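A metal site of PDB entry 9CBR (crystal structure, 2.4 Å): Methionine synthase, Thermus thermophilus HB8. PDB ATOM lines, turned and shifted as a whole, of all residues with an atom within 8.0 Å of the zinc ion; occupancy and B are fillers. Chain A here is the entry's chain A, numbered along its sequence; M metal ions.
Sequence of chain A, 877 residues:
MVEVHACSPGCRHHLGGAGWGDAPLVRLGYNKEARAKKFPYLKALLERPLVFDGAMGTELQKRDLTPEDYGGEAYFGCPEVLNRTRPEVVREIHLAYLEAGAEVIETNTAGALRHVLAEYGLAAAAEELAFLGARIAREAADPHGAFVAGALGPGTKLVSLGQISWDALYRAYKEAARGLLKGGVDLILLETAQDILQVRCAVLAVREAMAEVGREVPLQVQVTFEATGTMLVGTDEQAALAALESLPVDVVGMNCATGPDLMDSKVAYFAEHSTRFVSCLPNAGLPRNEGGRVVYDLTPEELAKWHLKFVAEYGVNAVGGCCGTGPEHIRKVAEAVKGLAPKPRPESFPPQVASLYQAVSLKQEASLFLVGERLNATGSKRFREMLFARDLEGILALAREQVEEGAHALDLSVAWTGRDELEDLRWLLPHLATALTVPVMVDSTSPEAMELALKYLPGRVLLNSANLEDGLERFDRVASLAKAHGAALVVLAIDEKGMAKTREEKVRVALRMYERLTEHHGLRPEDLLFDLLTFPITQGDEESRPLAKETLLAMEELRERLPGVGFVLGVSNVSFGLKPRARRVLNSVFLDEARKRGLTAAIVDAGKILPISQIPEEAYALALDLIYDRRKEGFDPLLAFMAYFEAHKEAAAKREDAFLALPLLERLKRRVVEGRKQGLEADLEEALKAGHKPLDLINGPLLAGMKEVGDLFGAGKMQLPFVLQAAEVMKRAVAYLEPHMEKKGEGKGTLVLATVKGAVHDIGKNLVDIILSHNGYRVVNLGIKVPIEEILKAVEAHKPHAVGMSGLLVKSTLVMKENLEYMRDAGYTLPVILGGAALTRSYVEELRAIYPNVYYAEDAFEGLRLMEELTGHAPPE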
ATOM      1  N   ALA A   6     -31.269  17.603  11.974  1.00  0.00           N
ATOM      2  CA  ALA A   6     -30.640  17.338  10.664  1.00  0.00           C
ATOM      3  C   ALA A   6     -29.720  16.122  10.757  1.00  0.00           C
ATOM      4  O   ALA A   6     -29.643  15.336   9.818  1.00  0.00           O
ATOM      5  CB  ALA A   6     -29.886  18.574  10.191  1.00  0.00           C
ATOM      6  N   CYS A   7     -29.026  15.964  11.909  1.00  0.00           N
ATOM      7  CA  CYS A   7     -28.068  14.879  12.121  1.00  0.00           C
ATOM      8  C   CYS A   7     -28.779  13.520  12.184  1.00  0.00           C
ATOM      9  O   CYS A   7     -29.998  13.456  12.297  1.00  0.00           O
ATOM     10  CB  CYS A   7     -27.172  15.118  13.350  1.00  0.00           C
ATOM     11  SG  CYS A   7     -25.776  16.257  13.076  1.00  0.00           S
ATOM     12  N   SER A   8     -27.990  12.434  12.042  1.00  0.00           N
ATOM     13  CA  SER A   8     -28.401  11.063  12.281  1.00  0.00           C
ATOM     14  C   SER A   8     -27.384  10.422  13.240  1.00  0.00           C
ATOM     15  O   SER A   8     -26.386  11.066  13.567  1.00  0.00           O
ATOM     16  CB  SER A   8     -28.509  10.308  10.956  1.00  0.00           C
ATOM     17  OG  SER A   8     -27.260   9.784  10.500  1.00  0.00           O
ATOM     18  N   PRO A   9     -27.580   9.178  13.755  1.00  0.00           N
ATOM     19  CA  PRO A   9     -26.565   8.536  14.589  1.00  0.00           C
ATOM     20  C   PRO A   9     -25.215   8.233  13.914  1.00  0.00           C
ATOM     21  O   PRO A   9     -24.240   7.935  14.609  1.00  0.00           O
ATOM     22  CB  PRO A   9     -27.241   7.276  15.126  1.00  0.00           C
ATOM     23  CG  PRO A   9     -28.673   7.318  14.652  1.00  0.00           C
ATOM     24  CD  PRO A   9     -28.802   8.372  13.602  1.00  0.00           C
ATOM     25  N   GLY A  10     -25.134   8.287  12.572  1.00  0.00           N
ATOM     26  CA  GLY A  10     -23.875   8.181  11.832  1.00  0.00           C
ATOM     27  C   GLY A  10     -22.969   9.402  11.989  1.00  0.00           C
ATOM     28  O   GLY A  10     -21.755   9.245  12.026  1.00  0.00           O
ATOM     29  N   CYS A  11     -23.562  10.595  12.077  1.00  0.00           N
ATOM     30  CA  CYS A  11     -22.824  11.846  12.142  1.00  0.00           C
ATOM     31  C   CYS A  11     -21.783  11.896  13.259  1.00  0.00           C
ATOM     32  O   CYS A  11     -22.019  11.414  14.366  1.00  0.00           O
ATOM     33  CB  CYS A  11     -23.751  13.014  12.461  1.00  0.00           C
ATOM     34  SG  CYS A  11     -25.018  13.366  11.232  1.00  0.00           S
ATOM     35  N   ARG A  12     -20.643  12.544  12.974  1.00  0.00           N
ATOM     36  CA  ARG A  12     -19.603  12.780  13.961  1.00  0.00           C
ATOM     37  C   ARG A  12     -18.750  13.971  13.506  1.00  0.00           C
ATOM     38  O   ARG A  12     -17.701  13.787  12.905  1.00  0.00           O
ATOM     39  CB  ARG A  12     -18.754  11.508  14.109  1.00  0.00           C
ATOM     40  CG  ARG A  12     -17.842  11.573  15.329  1.00  0.00           C
ATOM     41  CD  ARG A  12     -17.127  10.253  15.674  1.00  0.00           C
ATOM     42  NE  ARG A  12     -18.044   9.291  16.296  1.00  0.00           N
ATOM     43  CZ  ARG A  12     -18.796   8.429  15.619  1.00  0.00           C
ATOM     44  NH1 ARG A  12     -18.502   8.175  14.351  1.00  0.00           N
ATOM     45  NH2 ARG A  12     -19.813   7.807  16.206  1.00  0.00           N
ATOM     46  N   HIS A  13     -19.193  15.193  13.865  1.00  0.00           N
ATOM     47  CA  HIS A  13     -18.643  16.449  13.375  1.00  0.00           C
ATOM     48  C   HIS A  13     -17.616  17.060  14.331  1.00  0.00           C
ATOM     49  O   HIS A  13     -17.329  18.264  14.230  1.00  0.00           O
ATOM     50  CB  HIS A  13     -19.824  17.402  13.129  1.00  0.00           C
ATOM     51  CG  HIS A  13     -20.899  16.891  12.224  1.00  0.00           C
ATOM     52  ND1 HIS A  13     -20.660  16.316  10.999  1.00  0.00           N
ATOM     53  CD2 HIS A  13     -22.254  16.865  12.403  1.00  0.00           C
ATOM     54  CE1 HIS A  13     -21.839  15.951  10.463  1.00  0.00           C
ATOM     55  NE2 HIS A  13     -22.808  16.278  11.286  1.00  0.00           N
ATOM     56  N   ALA A  18     -18.657  20.540  10.999  1.00  0.00           N
ATOM     57  CA  ALA A  18     -19.826  20.426  10.147  1.00  0.00           C
ATOM     58  C   ALA A  18     -19.799  21.569   9.120  1.00  0.00           C
ATOM     59  O   ALA A  18     -18.784  22.264   8.982  1.00  0.00           O
ATOM     60  CB  ALA A  18     -21.069  20.464  10.981  1.00  0.00           C
ATOM     61  N   GLY A  19     -20.921  21.745   8.412  1.00  0.00           N
ATOM     62  CA  GLY A  19     -21.091  22.794   7.404  1.00  0.00           C
ATOM     63  C   GLY A  19     -21.577  24.129   7.946  1.00  0.00           C
ATOM     64  O   GLY A  19     -21.507  25.087   7.187  1.00  0.00           O
ATOM     65  N   TRP A  20     -22.065  24.189   9.200  1.00  0.00           N
ATOM     66  CA  TRP A  20     -22.539  25.399   9.864  1.00  0.00           C
ATOM     67  C   TRP A  20     -21.518  25.879  10.901  1.00  0.00           C
ATOM     68  O   TRP A  20     -20.684  25.104  11.369  1.00  0.00           O
ATOM     69  CB  TRP A  20     -23.929  25.208  10.510  1.00  0.00           C
ATOM     70  CG  TRP A  20     -24.046  24.064  11.490  1.00  0.00           C
ATOM     71  CD1 TRP A  20     -23.937  24.162  12.848  1.00  0.00           C
ATOM     72  CD2 TRP A  20     -24.305  22.672  11.200  1.00  0.00           C
ATOM     73  NE1 TRP A  20     -24.107  22.920  13.405  1.00  0.00           N
ATOM     74  CE2 TRP A  20     -24.320  21.993  12.431  1.00  0.00           C
ATOM     75  CE3 TRP A  20     -24.504  21.938  10.021  1.00  0.00           C
ATOM     76  CZ2 TRP A  20     -24.525  20.619  12.514  1.00  0.00           C
ATOM     77  CZ3 TRP A  20     -24.697  20.572  10.112  1.00  0.00           C
ATOM     78  CH2 TRP A  20     -24.686  19.905  11.342  1.00  0.00           C
ATOM     79  N   LEU A 472     -29.261   6.575   5.889  1.00  0.00           N
ATOM     80  CA  LEU A 472     -28.552   7.799   6.213  1.00  0.00           C
ATOM     81  C   LEU A 472     -27.402   7.619   7.217  1.00  0.00           C
ATOM     82  O   LEU A 472     -26.483   8.458   7.260  1.00  0.00           O
ATOM     83  CB  LEU A 472     -29.586   8.807   6.721  1.00  0.00           C
ATOM     84  CG  LEU A 472     -29.224  10.285   6.552  1.00  0.00           C
ATOM     85  CD1 LEU A 472     -29.234  10.734   5.106  1.00  0.00           C
ATOM     86  CD2 LEU A 472     -30.102  11.174   7.366  1.00  0.00           C
ATOM     87  N   ASP A 476     -23.679   9.208   6.360  1.00  0.00           N
ATOM     88  CA  ASP A 476     -23.105  10.229   7.230  1.00  0.00           C
ATOM     89  C   ASP A 476     -21.811   9.766   7.909  1.00  0.00           C
ATOM     90  O   ASP A 476     -20.896  10.582   8.063  1.00  0.00           O
ATOM     91  CB  ASP A 476     -24.097  10.732   8.250  1.00  0.00           C
ATOM     92  CG  ASP A 476     -25.352  11.386   7.672  1.00  0.00           C
ATOM     93  OD1 ASP A 476     -25.253  12.163   6.667  1.00  0.00           O
ATOM     94  OD2 ASP A 476     -26.436  11.161   8.271  1.00  0.00           O
ATOM     95  N   SER A 480     -18.428  11.890   7.406  1.00  0.00           N
ATOM     96  CA  SER A 480     -17.668  12.451   8.520  1.00  0.00           C
ATOM     97  C   SER A 480     -16.218  11.966   8.439  1.00  0.00           C
ATOM     98  O   SER A 480     -15.285  12.743   8.596  1.00  0.00           O
ATOM     99  CB  SER A 480     -18.269  12.084   9.877  1.00  0.00           C
ATOM    100  OG  SER A 480     -19.581  12.602  10.112  1.00  0.00           O
ATOM    101  N   ARG A 516     -26.586  17.010   1.167  1.00  0.00           N
ATOM    102  CA  ARG A 516     -26.080  16.511   2.423  1.00  0.00           C
ATOM    103  C   ARG A 516     -24.589  16.795   2.560  1.00  0.00           C
ATOM    104  O   ARG A 516     -24.153  17.202   3.620  1.00  0.00           O
ATOM    105  CB  ARG A 516     -26.297  15.012   2.638  1.00  0.00           C
ATOM    106  CG  ARG A 516     -27.737  14.572   2.844  1.00  0.00           C
ATOM    107  CD  ARG A 516     -28.276  14.911   4.230  1.00  0.00           C
ATOM    108  NE  ARG A 516     -27.775  14.175   5.390  1.00  0.00           N
ATOM    109  CZ  ARG A 516     -28.107  14.412   6.662  1.00  0.00           C
ATOM    110  NH1 ARG A 516     -28.980  15.337   6.984  1.00  0.00           N
ATOM    111  NH2 ARG A 516     -27.578  13.702   7.638  1.00  0.00           N
ATOM    112  N   HIS A 520     -24.566  20.201   4.874  1.00  0.00           N
ATOM    113  CA  HIS A 520     -24.533  19.571   6.187  1.00  0.00           C
ATOM    114  C   HIS A 520     -23.081  19.309   6.582  1.00  0.00           C
ATOM    115  O   HIS A 520     -22.577  19.940   7.505  1.00  0.00           O
ATOM    116  CB  HIS A 520     -25.455  18.333   6.223  1.00  0.00           C
ATOM    117  CG  HIS A 520     -25.595  17.749   7.576  1.00  0.00           C
ATOM    118  ND1 HIS A 520     -26.714  17.984   8.336  1.00  0.00           N
ATOM    119  CD2 HIS A 520     -24.798  17.010   8.355  1.00  0.00           C
ATOM    120  CE1 HIS A 520     -26.565  17.417   9.521  1.00  0.00           C
ATOM    121  NE2 HIS A 520     -25.403  16.832   9.550  1.00  0.00           N
ATOM    122  N   HIS A 521     -22.359  18.487   5.823  1.00  0.00           N
ATOM    123  CA  HIS A 521     -21.039  17.999   6.218  1.00  0.00           C
ATOM    124  C   HIS A 521     -19.915  18.965   5.856  1.00  0.00           C
ATOM    125  O   HIS A 521     -18.787  18.748   6.232  1.00  0.00           O
ATOM    126  CB  HIS A 521     -20.736  16.621   5.585  1.00  0.00           C
ATOM    127  CG  HIS A 521     -21.519  15.476   6.103  1.00  0.00           C
ATOM    128  ND1 HIS A 521     -21.018  14.658   7.089  1.00  0.00           N
ATOM    129  CD2 HIS A 521     -22.711  14.955   5.781  1.00  0.00           C
ATOM    130  CE1 HIS A 521     -21.909  13.711   7.373  1.00  0.00           C
ATOM    131  NE2 HIS A 521     -22.923  13.852   6.577  1.00  0.00           N
HETATM  132 ZN    ZN M   1     -24.732  15.644  11.076  1.00  0.00          ZN
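N of Gly 19 lies within hydrogen-bond range of O of His 520 (2.6 Å). SG of Cys 11 sits close to N of Ser 8, at 3.2 Å.
Four residues have an atom within 4 Å of the zinc ion: Cys 7, Cys 11, His 13 and His 520. The nearest printed residue that does not touch the zinc ion is Trp 20 (4.3 Å).
The zinc ion is bound by a ring nitrogen (NE2) of His 13 (2.0 Å), a ring nitrogen (NE2) of His 520 (2.0 Å), the side-chain sulfur (SG) of Cys 11 (2.3 Å) and the side-chain sulfur (SG) of Cys 7 (2.3 Å).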
